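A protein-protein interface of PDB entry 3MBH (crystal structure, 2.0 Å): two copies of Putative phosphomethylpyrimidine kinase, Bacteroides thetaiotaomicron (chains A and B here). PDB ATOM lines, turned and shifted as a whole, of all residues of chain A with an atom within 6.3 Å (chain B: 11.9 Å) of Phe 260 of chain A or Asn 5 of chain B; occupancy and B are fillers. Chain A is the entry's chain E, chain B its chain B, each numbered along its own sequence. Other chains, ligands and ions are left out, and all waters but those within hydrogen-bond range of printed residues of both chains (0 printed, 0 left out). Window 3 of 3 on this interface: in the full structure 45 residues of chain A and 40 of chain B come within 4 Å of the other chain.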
ATOM      1  N   ILE A 256      12.037  -4.513 -25.869  1.00  0.00           N
ATOM      2  CA  ILE A 256      13.309  -4.981 -26.399  1.00  0.00           C
ATOM      3  C   ILE A 256      14.411  -4.862 -25.331  1.00  0.00           C
ATOM      4  O   ILE A 256      15.180  -5.800 -25.116  1.00  0.00           O
ATOM      5  CB  ILE A 256      13.673  -4.239 -27.675  1.00  0.00           C
ATOM      6  CG1 ILE A 256      12.680  -4.639 -28.810  1.00  0.00           C
ATOM      7  CG2 ILE A 256      15.163  -4.541 -28.076  1.00  0.00           C
ATOM      8  CD1 ILE A 256      12.926  -3.889 -30.148  1.00  0.00           C
ATOM      9  N   ARG A 257      14.474  -3.737 -24.631  1.00  0.00           N
ATOM     10  CA  ARG A 257      15.509  -3.575 -23.621  1.00  0.00           C
ATOM     11  C   ARG A 257      15.408  -4.563 -22.474  1.00  0.00           C
ATOM     12  O   ARG A 257      16.452  -4.890 -21.877  1.00  0.00           O
ATOM     13  CB  ARG A 257      15.527  -2.145 -23.075  1.00  0.00           C
ATOM     14  CG  ARG A 257      16.006  -1.112 -24.106  1.00  0.00           C
ATOM     15  CD  ARG A 257      15.894   0.360 -23.563  1.00  0.00           C
ATOM     16  NE  ARG A 257      17.141   0.804 -22.905  1.00  0.00           N
ATOM     17  CZ  ARG A 257      17.347   0.887 -21.591  1.00  0.00           C
ATOM     18  NH1 ARG A 257      16.394   0.547 -20.738  1.00  0.00           N
ATOM     19  NH2 ARG A 257      18.528   1.319 -21.129  1.00  0.00           N
ATOM     20  N   ALA A 258      14.177  -5.012 -22.178  1.00  0.00           N
ATOM     21  CA  ALA A 258      13.916  -6.039 -21.192  1.00  0.00           C
ATOM     22  C   ALA A 258      14.564  -7.398 -21.569  1.00  0.00           C
ATOM     23  O   ALA A 258      14.800  -8.229 -20.686  1.00  0.00           O
ATOM     24  CB  ALA A 258      12.397  -6.221 -20.951  1.00  0.00           C
ATOM     25  N   THR A 259      14.901  -7.597 -22.849  1.00  0.00           N
ATOM     26  CA  THR A 259      15.563  -8.830 -23.254  1.00  0.00           C
ATOM     27  C   THR A 259      17.093  -8.776 -23.102  1.00  0.00           C
ATOM     28  O   THR A 259      17.757  -9.804 -23.273  1.00  0.00           O
ATOM     29  CB  THR A 259      15.213  -9.201 -24.727  1.00  0.00           C
ATOM     30  OG1 THR A 259      15.946  -8.323 -25.632  1.00  0.00           O
ATOM     31  CG2 THR A 259      13.719  -9.080 -24.959  1.00  0.00           C
ATOM     32  N   PHE A 260      17.661  -7.604 -22.785  1.00  0.00           N
ATOM     33  CA  PHE A 260      19.096  -7.454 -22.793  1.00  0.00           C
ATOM     34  C   PHE A 260      19.687  -8.013 -21.498  1.00  0.00           C
ATOM     35  O   PHE A 260      18.987  -8.138 -20.491  1.00  0.00           O
ATOM     36  CB  PHE A 260      19.542  -5.988 -22.989  1.00  0.00           C
ATOM     37  CG  PHE A 260      21.031  -5.826 -23.128  1.00  0.00           C
ATOM     38  CD1 PHE A 260      21.641  -5.929 -24.381  1.00  0.00           C
ATOM     39  CD2 PHE A 260      21.841  -5.642 -22.003  1.00  0.00           C
ATOM     40  CE1 PHE A 260      23.029  -5.837 -24.503  1.00  0.00           C
ATOM     41  CE2 PHE A 260      23.234  -5.514 -22.116  1.00  0.00           C
ATOM     42  CZ  PHE A 260      23.832  -5.610 -23.361  1.00  0.00           C
ATOM     43  N   GLY A 261      20.953  -8.402 -21.581  1.00  0.00           N
ATOM     44  CA  GLY A 261      21.783  -8.748 -20.405  1.00  0.00           C
ATOM     45  C   GLY A 261      22.048 -10.226 -20.224  1.00  0.00           C
ATOM     46  O   GLY A 261      22.891 -10.587 -19.424  1.00  0.00           O
ATOM     47  N   TYR A 262      21.289 -11.066 -20.937  1.00  0.00           N
ATOM     48  CA  TYR A 262      21.432 -12.514 -20.817  1.00  0.00           C
ATOM     49  C   TYR A 262      21.192 -13.107 -22.181  1.00  0.00           C
ATOM     50  O   TYR A 262      20.685 -12.406 -23.085  1.00  0.00           O
ATOM     51  CB  TYR A 262      20.411 -13.109 -19.815  1.00  0.00           C
ATOM     52  CG  TYR A 262      20.400 -12.437 -18.447  1.00  0.00           C
ATOM     53  CD1 TYR A 262      19.696 -11.246 -18.244  1.00  0.00           C
ATOM     54  CD2 TYR A 262      21.099 -12.979 -17.360  1.00  0.00           C
ATOM     55  CE1 TYR A 262      19.704 -10.599 -17.000  1.00  0.00           C
ATOM     56  CE2 TYR A 262      21.117 -12.326 -16.097  1.00  0.00           C
ATOM     57  CZ  TYR A 262      20.390 -11.148 -15.943  1.00  0.00           C
ATOM     58  OH  TYR A 262      20.362 -10.481 -14.739  1.00  0.00           O
ATOM     59  N   GLU A 263      21.514 -14.395 -22.314  1.00  0.00           N
ATOM     60  CA  GLU A 263      21.197 -15.176 -23.516  1.00  0.00           C
ATOM     61  C   GLU A 263      19.705 -15.061 -23.784  1.00  0.00           C
ATOM     62  O   GLU A 263      18.882 -15.331 -22.894  1.00  0.00           O
ATOM     63  CB  GLU A 263      21.629 -16.664 -23.324  1.00  0.00           C
ATOM     64  N   TYR A 264      19.325 -14.617 -24.981  1.00  0.00           N
ATOM     65  CA  TYR A 264      17.914 -14.521 -25.318  1.00  0.00           C
ATOM     66  C   TYR A 264      17.616 -15.009 -26.730  1.00  0.00           C
ATOM     67  O   TYR A 264      18.324 -14.695 -27.664  1.00  0.00           O
ATOM     68  CB  TYR A 264      17.447 -13.085 -25.167  1.00  0.00           C
ATOM     69  CG  TYR A 264      15.933 -12.948 -25.249  1.00  0.00           C
ATOM     70  CD1 TYR A 264      15.140 -13.234 -24.166  1.00  0.00           C
ATOM     71  CD2 TYR A 264      15.302 -12.517 -26.429  1.00  0.00           C
ATOM     72  CE1 TYR A 264      13.729 -13.099 -24.240  1.00  0.00           C
ATOM     73  CE2 TYR A 264      13.905 -12.349 -26.498  1.00  0.00           C
ATOM     74  CZ  TYR A 264      13.128 -12.648 -25.403  1.00  0.00           C
ATOM     75  OH  TYR A 264      11.757 -12.517 -25.455  1.00  0.00           O
ATOM     76  N   LEU A 271       9.749  -8.880 -24.720  1.00  0.00           N
ATOM     77  CA  LEU A 271       9.281  -9.487 -23.479  1.00  0.00           C
ATOM     78  C   LEU A 271       7.999  -8.776 -23.066  1.00  0.00           C
ATOM     79  O   LEU A 271       7.940  -8.082 -22.056  1.00  0.00           O
ATOM     80  CB  LEU A 271      10.318  -9.462 -22.342  1.00  0.00           C
ATOM     81  CG  LEU A 271      11.141 -10.679 -21.881  1.00  0.00           C
ATOM     82  CD1 LEU A 271      11.655 -10.401 -20.436  1.00  0.00           C
ATOM     83  CD2 LEU A 271      10.459 -12.044 -21.995  1.00  0.00           C
ATOM     84  N   ASN B   5      15.686 -11.881 -17.553  1.00  0.00           N
ATOM     85  CA  ASN B   5      14.999 -11.656 -18.856  1.00  0.00           C
ATOM     86  C   ASN B   5      14.137 -12.889 -19.328  1.00  0.00           C
ATOM     87  O   ASN B   5      14.080 -13.212 -20.544  1.00  0.00           O
ATOM     88  CB  ASN B   5      15.974 -11.068 -19.943  1.00  0.00           C
ATOM     89  CG  ASN B   5      17.005 -12.097 -20.550  1.00  0.00           C
ATOM     90  OD1 ASN B   5      16.895 -13.318 -20.405  1.00  0.00           O
ATOM     91  ND2 ASN B   5      18.007 -11.559 -21.259  1.00  0.00           N
ATOM     92  N   LYS B   6      13.461 -13.554 -18.366  1.00  0.00           N
ATOM     93  CA  LYS B   6      12.550 -14.689 -18.676  1.00  0.00           C
ATOM     94  C   LYS B   6      11.146 -14.522 -18.092  1.00  0.00           C
ATOM     95  O   LYS B   6      10.925 -14.033 -17.008  1.00  0.00           O
ATOM     96  CB  LYS B   6      13.107 -16.035 -18.251  1.00  0.00           C
ATOM     97  CG  LYS B   6      12.522 -17.201 -19.074  1.00  0.00           C
ATOM     98  CD  LYS B   6      12.658 -18.576 -18.382  1.00  0.00           C
ATOM     99  CE  LYS B   6      11.438 -19.501 -18.708  1.00  0.00           C
ATOM    100  NZ  LYS B   6      10.777 -19.277 -20.049  1.00  0.00           N
ATOM    101  N   VAL B   7      10.187 -14.910 -18.897  1.00  0.00           N
ATOM    102  CA  VAL B   7       8.804 -14.855 -18.542  1.00  0.00           C
ATOM    103  C   VAL B   7       8.379 -16.313 -18.658  1.00  0.00           C
ATOM    104  O   VAL B   7       8.612 -16.942 -19.689  1.00  0.00           O
ATOM    105  CB  VAL B   7       8.089 -13.961 -19.570  1.00  0.00           C
ATOM    106  CG1 VAL B   7       6.624 -14.288 -19.655  1.00  0.00           C
ATOM    107  CG2 VAL B   7       8.374 -12.483 -19.251  1.00  0.00           C
ATOM    108  N   LYS B   8       7.800 -16.858 -17.597  1.00  0.00           N
ATOM    109  CA  LYS B   8       7.291 -18.234 -17.587  1.00  0.00           C
ATOM    110  C   LYS B   8       6.165 -18.422 -18.614  1.00  0.00           C
ATOM    111  O   LYS B   8       5.387 -17.516 -18.811  1.00  0.00           O
ATOM    112  CB  LYS B   8       6.773 -18.600 -16.188  1.00  0.00           C
ATOM    113  CG  LYS B   8       7.912 -18.724 -15.187  1.00  0.00           C
ATOM    114  CD  LYS B   8       7.482 -19.357 -13.884  1.00  0.00           C
ATOM    115  CE  LYS B   8       8.721 -19.471 -12.995  1.00  0.00           C
ATOM    116  NZ  LYS B   8       8.420 -20.108 -11.729  1.00  0.00           N
ATOM    117  N   LYS B   9       6.138 -19.586 -19.262  1.00  0.00           N
ATOM    118  CA  LYS B   9       5.186 -19.923 -20.328  1.00  0.00           C
ATOM    119  C   LYS B   9       4.173 -20.941 -19.797  1.00  0.00           C
ATOM    120  O   LYS B   9       4.542 -21.886 -19.076  1.00  0.00           O
ATOM    121  CB  LYS B   9       5.875 -20.611 -21.529  1.00  0.00           C
ATOM    122  CG  LYS B   9       6.922 -19.794 -22.323  1.00  0.00           C
ATOM    123  CD  LYS B   9       7.509 -20.675 -23.489  1.00  0.00           C
ATOM    124  CE  LYS B   9       8.951 -20.413 -23.816  1.00  0.00           C
ATOM    125  NZ  LYS B   9       9.559 -19.010 -23.419  1.00  0.00           N
ATOM    126  N   GLY B  35       1.680 -11.684 -15.661  1.00  0.00           N
ATOM    127  CA  GLY B  35       3.133 -11.749 -15.944  1.00  0.00           C
ATOM    128  C   GLY B  35       3.550 -13.018 -16.640  1.00  0.00           C
ATOM    129  O   GLY B  35       4.724 -13.280 -16.734  1.00  0.00           O
ATOM    130  N   PHE B  36       2.609 -13.801 -17.150  1.00  0.00           N
ATOM    131  CA  PHE B  36       2.951 -15.040 -17.837  1.00  0.00           C
ATOM    132  C   PHE B  36       2.646 -15.045 -19.357  1.00  0.00           C
ATOM    133  O   PHE B  36       1.609 -14.546 -19.802  1.00  0.00           O
ATOM    134  CB  PHE B  36       2.212 -16.203 -17.155  1.00  0.00           C
ATOM    135  CG  PHE B  36       2.398 -16.221 -15.676  1.00  0.00           C
ATOM    136  CD1 PHE B  36       3.637 -16.553 -15.135  1.00  0.00           C
ATOM    137  CD2 PHE B  36       1.414 -15.766 -14.831  1.00  0.00           C
ATOM    138  CE1 PHE B  36       3.853 -16.503 -13.760  1.00  0.00           C
ATOM    139  CE2 PHE B  36       1.612 -15.737 -13.441  1.00  0.00           C
ATOM    140  CZ  PHE B  36       2.844 -16.105 -12.908  1.00  0.00           C
ATOM    141  N   GLN B  37       3.483 -15.712 -20.132  1.00  0.00           N
ATOM    142  CA  GLN B  37       3.195 -15.857 -21.538  1.00  0.00           C
ATOM    143  C   GLN B  37       2.233 -17.046 -21.670  1.00  0.00           C
ATOM    144  O   GLN B  37       2.504 -18.132 -21.132  1.00  0.00           O
ATOM    145  CB  GLN B  37       4.456 -16.110 -22.361  1.00  0.00           C
ATOM    146  CG  GLN B  37       4.119 -16.299 -23.849  1.00  0.00           C
ATOM    147  CD  GLN B  37       5.335 -16.570 -24.706  1.00  0.00           C
ATOM    148  OE1 GLN B  37       6.455 -16.746 -24.220  1.00  0.00           O
ATOM    149  NE2 GLN B  37       5.103 -16.585 -26.014  1.00  0.00           N
ATOM    150  N   ASP B  79       6.269 -24.028 -18.126  1.00  0.00           N
ATOM    151  CA  ASP B  79       6.230 -23.955 -16.667  1.00  0.00           C
ATOM    152  C   ASP B  79       4.848 -24.438 -16.157  1.00  0.00           C
ATOM    153  O   ASP B  79       4.739 -24.941 -15.063  1.00  0.00           O
ATOM    154  CB  ASP B  79       6.558 -22.528 -16.231  1.00  0.00           C
ATOM    155  CG  ASP B  79       7.935 -22.053 -16.772  1.00  0.00           C
ATOM    156  OD1 ASP B  79       8.993 -22.446 -16.208  1.00  0.00           O
ATOM    157  OD2 ASP B  79       7.991 -21.377 -17.821  1.00  0.00           O
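No position is printed for both chains.
O of Ile 256 of chain A lies within hydrogen-bond range of OG1 of Thr 259 of chain A, 2.7 Å away.
Of the printed residues of chain B, Phe 260 of chain A touches Asn 5 (3.6 Å).
Printed residues of chain A within 4 Å of Asn 5 of chain B: Ala 258 (3.2 Å), Thr 259 (2.7 Å), Phe 260 (3.6 Å), Tyr 262 (3.2 Å), Glu 263 (3.8 Å), Tyr 264 (3.7 Å) and Leu 271 (3.7 Å).
Of chain B, only Asn 5 (3.2 Å) comes within 4 Å of Ala 258 of chain A.
Tyr 262 of chain A touches one residue of chain B.
Of chain B, only Asn 5 (3.7 Å) comes within 4 Å of Tyr 264 of chain A.
Printed residues of chain A within 4 Å of Val 7 of chain B: Leu 271 (3.5 Å).
Printed residues of chain B within 4 Å of Leu 271 of chain A: Asn 5 (3.7 Å) and Val 7 (3.5 Å).
The nearest printed residue of chain A that does not touch Asn 5 of chain B is Gly 261 of chain A (4.3 Å).
Hydrophobic or aromatic side chains of chain B that line the printed part of chain A: Val 7.
Among the printed residues, 8 pairs touch across the chains.
Asn 5 of chain B touches Ala 258 of chain A (CB to O, 3.2 Å).
O of Phe 260 of chain A touches ND2 of Asn 5 of chain B (3.6 Å).
Asn 5 of chain B touches Glu 263 of chain A (OD1 to O, 3.8 Å).
Tyr 264 of chain A touches Asn 5 of chain B.
Asn 5 of chain B touches Leu 271 of chain A (C to CD1, 3.7 Å).
Leu 271 of chain A touches Val 7 of chain B.
ND2 of Asn 5 of chain B is in hydrogen-bond range of O of Thr 259 of chain A (2.7 Å).
ND2 of Asn 5 of chain B lies close to N of Tyr 262 of chain A (3.3 Å).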
